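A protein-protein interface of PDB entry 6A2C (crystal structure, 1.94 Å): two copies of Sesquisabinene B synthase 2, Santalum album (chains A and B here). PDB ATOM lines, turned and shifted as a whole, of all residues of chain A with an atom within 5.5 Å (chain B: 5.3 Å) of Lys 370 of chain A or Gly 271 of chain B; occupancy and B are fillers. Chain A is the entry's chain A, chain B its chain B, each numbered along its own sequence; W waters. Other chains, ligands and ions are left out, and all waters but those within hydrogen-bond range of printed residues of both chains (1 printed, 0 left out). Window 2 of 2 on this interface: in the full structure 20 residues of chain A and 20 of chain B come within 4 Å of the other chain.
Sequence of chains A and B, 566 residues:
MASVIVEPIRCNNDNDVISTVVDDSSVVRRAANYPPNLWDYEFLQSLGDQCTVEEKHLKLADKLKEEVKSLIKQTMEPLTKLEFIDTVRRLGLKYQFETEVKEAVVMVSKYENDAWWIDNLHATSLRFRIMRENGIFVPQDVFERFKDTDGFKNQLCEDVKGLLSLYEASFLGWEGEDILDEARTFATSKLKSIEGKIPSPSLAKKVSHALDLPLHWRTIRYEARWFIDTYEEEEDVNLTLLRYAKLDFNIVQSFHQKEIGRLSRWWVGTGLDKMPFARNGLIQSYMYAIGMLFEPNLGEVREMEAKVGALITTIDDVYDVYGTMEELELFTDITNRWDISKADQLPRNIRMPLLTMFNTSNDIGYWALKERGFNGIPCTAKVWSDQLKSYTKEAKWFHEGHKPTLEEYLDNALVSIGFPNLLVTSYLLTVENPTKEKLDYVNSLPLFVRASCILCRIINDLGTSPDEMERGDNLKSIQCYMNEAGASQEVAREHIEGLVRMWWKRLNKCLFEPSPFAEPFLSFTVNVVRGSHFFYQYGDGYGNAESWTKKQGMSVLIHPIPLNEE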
ATOM      1  N   GLU A 300     -28.059   3.197   4.694  1.00  0.00           N
ATOM      2  CA  GLU A 300     -27.250   2.013   5.071  1.00  0.00           C
ATOM      3  C   GLU A 300     -26.525   2.290   6.396  1.00  0.00           C
ATOM      4  O   GLU A 300     -26.447   1.357   7.252  1.00  0.00           O
ATOM      5  CB  GLU A 300     -26.256   1.613   3.984  1.00  0.00           C
ATOM      6  CG  GLU A 300     -26.915   0.932   2.807  1.00  0.00           C
ATOM      7  CD  GLU A 300     -25.919   0.249   1.889  1.00  0.00           C
ATOM      8  OE1 GLU A 300     -25.379   0.926   1.001  1.00  0.00           O
ATOM      9  OE2 GLU A 300     -25.622  -0.936   2.134  1.00  0.00           O
ATOM     10  N   TYR A 366     -16.920  -5.686   7.410  1.00  0.00           N
ATOM     11  CA  TYR A 366     -16.876  -6.227   6.029  1.00  0.00           C
ATOM     12  C   TYR A 366     -17.517  -5.211   5.070  1.00  0.00           C
ATOM     13  O   TYR A 366     -17.016  -5.046   3.937  1.00  0.00           O
ATOM     14  CB  TYR A 366     -17.533  -7.601   5.941  1.00  0.00           C
ATOM     15  CG  TYR A 366     -17.497  -8.147   4.538  1.00  0.00           C
ATOM     16  CD1 TYR A 366     -18.441  -7.776   3.605  1.00  0.00           C
ATOM     17  CD2 TYR A 366     -16.444  -8.940   4.127  1.00  0.00           C
ATOM     18  CE1 TYR A 366     -18.390  -8.253   2.303  1.00  0.00           C
ATOM     19  CE2 TYR A 366     -16.389  -9.451   2.841  1.00  0.00           C
ATOM     20  CZ  TYR A 366     -17.341  -9.065   1.915  1.00  0.00           C
ATOM     21  OH  TYR A 366     -17.279  -9.523   0.638  1.00  0.00           O
ATOM     22  N   TRP A 367     -18.597  -4.556   5.471  1.00  0.00           N
ATOM     23  CA  TRP A 367     -19.222  -3.498   4.641  1.00  0.00           C
ATOM     24  C   TRP A 367     -18.170  -2.426   4.308  1.00  0.00           C
ATOM     25  O   TRP A 367     -18.105  -1.995   3.127  1.00  0.00           O
ATOM     26  CB  TRP A 367     -20.432  -2.906   5.339  1.00  0.00           C
ATOM     27  CG  TRP A 367     -21.225  -1.939   4.519  1.00  0.00           C
ATOM     28  CD1 TRP A 367     -22.394  -2.186   3.876  1.00  0.00           C
ATOM     29  CD2 TRP A 367     -20.949  -0.539   4.320  1.00  0.00           C
ATOM     30  NE1 TRP A 367     -22.886  -1.039   3.319  1.00  0.00           N
ATOM     31  CE2 TRP A 367     -22.015  -0.011   3.569  1.00  0.00           C
ATOM     32  CE3 TRP A 367     -19.950   0.322   4.766  1.00  0.00           C
ATOM     33  CZ2 TRP A 367     -22.078   1.334   3.204  1.00  0.00           C
ATOM     34  CZ3 TRP A 367     -20.013   1.653   4.414  1.00  0.00           C
ATOM     35  CH2 TRP A 367     -21.076   2.153   3.658  1.00  0.00           C
ATOM     36  N   ALA A 368     -17.373  -1.991   5.284  1.00  0.00           N
ATOM     37  CA  ALA A 368     -16.311  -0.994   5.052  1.00  0.00           C
ATOM     38  C   ALA A 368     -15.295  -1.540   4.036  1.00  0.00           C
ATOM     39  O   ALA A 368     -14.801  -0.750   3.201  1.00  0.00           O
ATOM     40  CB  ALA A 368     -15.645  -0.604   6.340  1.00  0.00           C
ATOM     41  N   LEU A 369     -14.980  -2.836   4.074  1.00  0.00           N
ATOM     42  CA  LEU A 369     -14.063  -3.433   3.074  1.00  0.00           C
ATOM     43  C   LEU A 369     -14.708  -3.391   1.688  1.00  0.00           C
ATOM     44  O   LEU A 369     -14.016  -2.969   0.742  1.00  0.00           O
ATOM     45  CB  LEU A 369     -13.685  -4.865   3.446  1.00  0.00           C
ATOM     46  CG  LEU A 369     -12.886  -5.590   2.368  1.00  0.00           C
ATOM     47  CD1 LEU A 369     -11.580  -4.861   2.091  1.00  0.00           C
ATOM     48  CD2 LEU A 369     -12.642  -7.031   2.749  1.00  0.00           C
ATOM     49  N   LYS A 370     -15.936  -3.880   1.567  1.00  0.00           N
ATOM     50  CA  LYS A 370     -16.667  -4.047   0.290  1.00  0.00           C
ATOM     51  C   LYS A 370     -16.927  -2.658  -0.299  1.00  0.00           C
ATOM     52  O   LYS A 370     -16.718  -2.443  -1.508  1.00  0.00           O
ATOM     53  CB  LYS A 370     -17.964  -4.804   0.595  1.00  0.00           C
ATOM     54  CG  LYS A 370     -19.020  -4.816  -0.489  1.00  0.00           C
ATOM     55  CD  LYS A 370     -19.830  -3.553  -0.579  1.00  0.00           C
ATOM     56  CE  LYS A 370     -21.065  -3.506   0.289  1.00  0.00           C
ATOM     57  NZ  LYS A 370     -22.024  -2.505  -0.240  1.00  0.00           N
ATOM     58  N   GLU A 371     -17.377  -1.733   0.542  1.00  0.00           N
ATOM     59  CA  GLU A 371     -17.914  -0.439   0.083  1.00  0.00           C
ATOM     60  C   GLU A 371     -16.812   0.612   0.097  1.00  0.00           C
ATOM     61  O   GLU A 371     -16.803   1.455  -0.815  1.00  0.00           O
ATOM     62  CB  GLU A 371     -19.110  -0.030   0.928  1.00  0.00           C
ATOM     63  CG  GLU A 371     -19.834   1.175   0.376  1.00  0.00           C
ATOM     64  CD  GLU A 371     -20.485   0.963  -0.989  1.00  0.00           C
ATOM     65  OE1 GLU A 371     -20.732  -0.194  -1.370  1.00  0.00           O
ATOM     66  OE2 GLU A 371     -20.786   1.963  -1.634  1.00  0.00           O
ATOM     67  N   ARG A 372     -15.948   0.609   1.109  1.00  0.00           N
ATOM     68  CA  ARG A 372     -15.079   1.778   1.395  1.00  0.00           C
ATOM     69  C   ARG A 372     -13.620   1.398   1.136  1.00  0.00           C
ATOM     70  O   ARG A 372     -12.796   2.277   1.295  1.00  0.00           O
ATOM     71  CB  ARG A 372     -15.302   2.330   2.812  1.00  0.00           C
ATOM     72  CG  ARG A 372     -16.758   2.533   3.226  1.00  0.00           C
ATOM     73  CD  ARG A 372     -17.537   3.564   2.417  1.00  0.00           C
ATOM     74  NE  ARG A 372     -16.992   4.887   2.618  1.00  0.00           N
ATOM     75  CZ  ARG A 372     -17.197   5.925   1.817  1.00  0.00           C
ATOM     76  NH1 ARG A 372     -18.015   5.815   0.783  1.00  0.00           N
ATOM     77  NH2 ARG A 372     -16.588   7.081   2.062  1.00  0.00           N
ATOM     78  N   GLY A 373     -13.367   0.159   0.701  1.00  0.00           N
ATOM     79  CA  GLY A 373     -12.048  -0.437   0.418  1.00  0.00           C
ATOM     80  C   GLY A 373     -11.239  -0.781   1.655  1.00  0.00           C
ATOM     81  O   GLY A 373     -10.073  -1.143   1.498  1.00  0.00           O
ATOM     82  N   PHE A 374     -11.784  -0.639   2.868  1.00  0.00           N
ATOM     83  CA  PHE A 374     -10.978  -0.821   4.103  1.00  0.00           C
ATOM     84  C   PHE A 374     -11.670  -1.811   5.048  1.00  0.00           C
ATOM     85  O   PHE A 374     -12.864  -1.644   5.322  1.00  0.00           O
ATOM     86  CB  PHE A 374     -10.722   0.533   4.751  1.00  0.00           C
ATOM     87  CG  PHE A 374      -9.987   0.489   6.061  1.00  0.00           C
ATOM     88  CD1 PHE A 374      -8.610   0.412   6.105  1.00  0.00           C
ATOM     89  CD2 PHE A 374     -10.686   0.578   7.250  1.00  0.00           C
ATOM     90  CE1 PHE A 374      -7.944   0.385   7.315  1.00  0.00           C
ATOM     91  CE2 PHE A 374     -10.022   0.545   8.457  1.00  0.00           C
ATOM     92  CZ  PHE A 374      -8.653   0.434   8.488  1.00  0.00           C
ATOM     93  N   TRP B 267     -26.260 -11.101  -1.793  1.00  0.00           N
ATOM     94  CA  TRP B 267     -25.139 -11.288  -2.744  1.00  0.00           C
ATOM     95  C   TRP B 267     -24.532  -9.935  -3.113  1.00  0.00           C
ATOM     96  O   TRP B 267     -23.331  -9.841  -3.081  1.00  0.00           O
ATOM     97  CB  TRP B 267     -25.622 -12.021  -3.998  1.00  0.00           C
ATOM     98  CG  TRP B 267     -24.551 -12.513  -4.909  1.00  0.00           C
ATOM     99  CD1 TRP B 267     -24.475 -12.291  -6.257  1.00  0.00           C
ATOM    100  CD2 TRP B 267     -23.476 -13.414  -4.585  1.00  0.00           C
ATOM    101  NE1 TRP B 267     -23.357 -12.892  -6.766  1.00  0.00           N
ATOM    102  CE2 TRP B 267     -22.767 -13.650  -5.786  1.00  0.00           C
ATOM    103  CE3 TRP B 267     -23.057 -14.074  -3.421  1.00  0.00           C
ATOM    104  CZ2 TRP B 267     -21.673 -14.510  -5.846  1.00  0.00           C
ATOM    105  CZ3 TRP B 267     -21.964 -14.910  -3.478  1.00  0.00           C
ATOM    106  CH2 TRP B 267     -21.289 -15.132  -4.676  1.00  0.00           C
ATOM    107  N   VAL B 268     -25.353  -8.955  -3.474  1.00  0.00           N
ATOM    108  CA  VAL B 268     -24.850  -7.610  -3.898  1.00  0.00           C
ATOM    109  C   VAL B 268     -24.163  -6.956  -2.696  1.00  0.00           C
ATOM    110  O   VAL B 268     -23.037  -6.408  -2.862  1.00  0.00           O
ATOM    111  CB  VAL B 268     -25.974  -6.745  -4.504  1.00  0.00           C
ATOM    112  CG1 VAL B 268     -25.585  -5.279  -4.543  1.00  0.00           C
ATOM    113  CG2 VAL B 268     -26.346  -7.217  -5.896  1.00  0.00           C
ATOM    114  N   GLY B 269     -24.709  -7.185  -1.492  1.00  0.00           N
ATOM    115  CA  GLY B 269     -24.105  -6.709  -0.229  1.00  0.00           C
ATOM    116  C   GLY B 269     -22.743  -7.317   0.042  1.00  0.00           C
ATOM    117  O   GLY B 269     -21.898  -6.655   0.692  1.00  0.00           O
ATOM    118  N   THR B 270     -22.460  -8.504  -0.483  1.00  0.00           N
ATOM    119  CA  THR B 270     -21.112  -9.117  -0.321  1.00  0.00           C
ATOM    120  C   THR B 270     -20.104  -8.511  -1.299  1.00  0.00           C
ATOM    121  O   THR B 270     -18.928  -8.628  -1.044  1.00  0.00           O
ATOM    122  CB  THR B 270     -21.150 -10.641  -0.497  1.00  0.00           C
ATOM    123  OG1 THR B 270     -21.341 -10.974  -1.870  1.00  0.00           O
ATOM    124  CG2 THR B 270     -22.188 -11.319   0.366  1.00  0.00           C
ATOM    125  N   GLY B 271     -20.568  -7.931  -2.401  1.00  0.00           N
ATOM    126  CA  GLY B 271     -19.649  -7.430  -3.440  1.00  0.00           C
ATOM    127  C   GLY B 271     -19.103  -8.542  -4.328  1.00  0.00           C
ATOM    128  O   GLY B 271     -18.291  -8.239  -5.196  1.00  0.00           O
ATOM    129  N   LEU B 272     -19.564  -9.781  -4.145  1.00  0.00           N
ATOM    130  CA  LEU B 272     -18.995 -10.926  -4.896  1.00  0.00           C
ATOM    131  C   LEU B 272     -19.597 -11.005  -6.305  1.00  0.00           C
ATOM    132  O   LEU B 272     -19.087 -11.772  -7.113  1.00  0.00           O
ATOM    133  CB  LEU B 272     -19.199 -12.211  -4.096  1.00  0.00           C
ATOM    134  CG  LEU B 272     -18.433 -12.302  -2.777  1.00  0.00           C
ATOM    135  CD1 LEU B 272     -18.526 -13.698  -2.195  1.00  0.00           C
ATOM    136  CD2 LEU B 272     -16.984 -11.893  -2.947  1.00  0.00           C
ATOM    137  N   ASP B 273     -20.643 -10.236  -6.567  1.00  0.00           N
ATOM    138  CA  ASP B 273     -21.250 -10.178  -7.920  1.00  0.00           C
ATOM    139  C   ASP B 273     -20.321  -9.372  -8.825  1.00  0.00           C
ATOM    140  O   ASP B 273     -20.378  -9.566 -10.046  1.00  0.00           O
ATOM    141  CB  ASP B 273     -22.624  -9.517  -7.856  1.00  0.00           C
ATOM    142  CG  ASP B 273     -22.632  -8.137  -7.232  1.00  0.00           C
ATOM    143  OD1 ASP B 273     -22.065  -7.986  -6.146  1.00  0.00           O
ATOM    144  OD2 ASP B 273     -23.215  -7.230  -7.839  1.00  0.00           O
ATOM    145  N   LYS B 274     -19.490  -8.525  -8.227  1.00  0.00           N
ATOM    146  CA  LYS B 274     -18.602  -7.630  -9.005  1.00  0.00           C
ATOM    147  C   LYS B 274     -17.225  -8.269  -9.068  1.00  0.00           C
ATOM    148  O   LYS B 274     -16.276  -7.606  -9.490  1.00  0.00           O
ATOM    149  CB  LYS B 274     -18.552  -6.261  -8.327  1.00  0.00           C
ATOM    150  CG  LYS B 274     -19.838  -5.455  -8.398  1.00  0.00           C
ATOM    151  CD  LYS B 274     -19.695  -4.077  -7.800  1.00  0.00           C
ATOM    152  CE  LYS B 274     -20.840  -3.158  -8.163  1.00  0.00           C
ATOM    153  NZ  LYS B 274     -21.811  -3.021  -7.054  1.00  0.00           N
ATOM    154  N   MET B 275     -17.141  -9.519  -8.643  1.00  0.00           N
ATOM    155  CA  MET B 275     -15.843 -10.219  -8.681  1.00  0.00           C
ATOM    156  C   MET B 275     -15.582 -10.695 -10.099  1.00  0.00           C
ATOM    157  O   MET B 275     -16.540 -11.106 -10.773  1.00  0.00           O
ATOM    158  CB  MET B 275     -15.829 -11.464  -7.797  1.00  0.00           C
ATOM    159  CG  MET B 275     -15.788 -11.168  -6.317  1.00  0.00           C
ATOM    160  SD  MET B 275     -14.193 -10.680  -5.654  1.00  0.00           S
ATOM    161  CE  MET B 275     -14.441  -8.916  -5.466  1.00  0.00           C
ATOM    162  N   ARG B 348      -7.856  -7.978  -2.000  1.00  0.00           N
ATOM    163  CA  ARG B 348      -9.307  -7.697  -1.998  1.00  0.00           C
ATOM    164  C   ARG B 348     -10.091  -8.892  -2.545  1.00  0.00           C
ATOM    165  O   ARG B 348     -11.078  -9.308  -1.878  1.00  0.00           O
ATOM    166  CB  ARG B 348      -9.576  -6.438  -2.830  1.00  0.00           C
ATOM    167  CG  ARG B 348     -11.030  -5.989  -2.820  1.00  0.00           C
ATOM    168  CD  ARG B 348     -11.344  -4.840  -3.771  1.00  0.00           C
ATOM    169  NE  ARG B 348     -12.782  -4.582  -3.814  1.00  0.00           N
ATOM    170  CZ  ARG B 348     -13.481  -4.026  -2.819  1.00  0.00           C
ATOM    171  NH1 ARG B 348     -12.863  -3.605  -1.724  1.00  0.00           N
ATOM    172  NH2 ARG B 348     -14.781  -3.841  -2.951  1.00  0.00           N
ATOM    173  N   MET B 352     -12.322 -10.946   0.256  1.00  0.00           N
ATOM    174  CA  MET B 352     -13.794 -10.803   0.236  1.00  0.00           C
ATOM    175  C   MET B 352     -14.464 -12.177   0.220  1.00  0.00           C
ATOM    176  O   MET B 352     -15.277 -12.466   1.106  1.00  0.00           O
ATOM    177  CB  MET B 352     -14.238  -9.873  -0.902  1.00  0.00           C
ATOM    178  CG  MET B 352     -14.026  -8.412  -0.509  1.00  0.00           C
ATOM    179  SD  MET B 352     -14.346  -7.133  -1.753  1.00  0.00           S
ATOM    180  CE  MET B 352     -16.067  -7.378  -2.163  1.00  0.00           C
HETATM  181  O   HOH W   1     -22.841  -3.465  -2.675  1.00  0.00           O
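The backbone carbonyl oxygen (O) of Lys 370 of chain A sits at hydrogen-bond distance from the guanidinium group (NH2) of Arg 348 of chain B (2.8 Å). The backbone carbonyl oxygen of Thr 270 of chain B lies within hydrogen-bond range of the side-chain hydroxyl of Tyr 366 of chain A. O of Leu 369 of chain A sits at hydrogen-bond distance from NH1 of Arg 348 of chain B (2.8 Å).
The side-chain hydroxyl (OG1) of Thr 270 of chain B lies within hydrogen-bond range of the backbone NH (N) of Leu 272 of chain B, 3.1 Å away. NH2 of Arg 348 of chain B sits close to SD of Met 352 of chain B (3.5 Å). The backbone carbonyl oxygen of Phe 374 of chain A sits at hydrogen-bond distance from the backbone NH of Leu 369 of chain A (2.7 Å). The backbone NH (N) of Gly 373 of chain A is in hydrogen-bond range of the backbone carbonyl oxygen (O) of Ala 368 of chain A (3.0 Å). O of Trp 267 of chain B sits at hydrogen-bond distance from OG1 of Thr 270 of chain B (2.6 Å). The side-chain amino group of Lys 370 of chain A lies within salt-bridge range of the side-chain carboxylate of Glu 371 of chain A (2.9 Å).
Among the printed residues, merely in contact across the chains: Tyr 366 of chain A with Met 352 of chain B (3.4 Å), Leu 369 of chain A with Met 352 of chain B (3.8 Å), Lys 370 of chain A with Gly 269 of chain B (3.3 Å), Lys 370 of chain A with Thr 270 of chain B (3.9 Å), Lys 370 of chain A with Gly 271 of chain B (3.97 Å) and Gly 373 of chain A with Arg 348 of chain B (3.9 Å).
Gly 271 of chain B touches just one residue of chain A: Lys 370. Printed residues of chain A within 4 Å of Thr 270 of chain B: Tyr 366 and Lys 370. Printed residues of chain A within 4 Å of Gly 269 of chain B: Lys 370. Of the printed residues of chain B, Gly 373 of chain A touches Arg 348 (3.9 Å). Trp 367 of chain A touches none of the printed residues of chain B. Glu 371 of chain A touches none of the printed residues of chain B. The nearest residue of chain B that does not touch Lys 370 of chain A is Met 352 of chain B (4.2 Å).
Of the 10 printed residues of chain A, 4 touch a printed residue of chain B. Hydrophobic or aromatic side chains of chain B within 4 Å of the printed part of chain A: Met 352. Among the printed residues, no Asp or Glu carboxylate lies within 4 Å of a Lys or Arg side-chain nitrogen of the other chain.
No position is printed for both chains. Of the 9 pairs that touch across the chains among the printed residues, none has its exchanged pair printed and touching as well.
Water W1 lies within hydrogen-bond range of the side-chain amino group (NZ) of Lys 370 of chain A (2.7 Å) and the backbone carbonyl oxygen (O) of Val 268 of chain B (3.0 Å).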
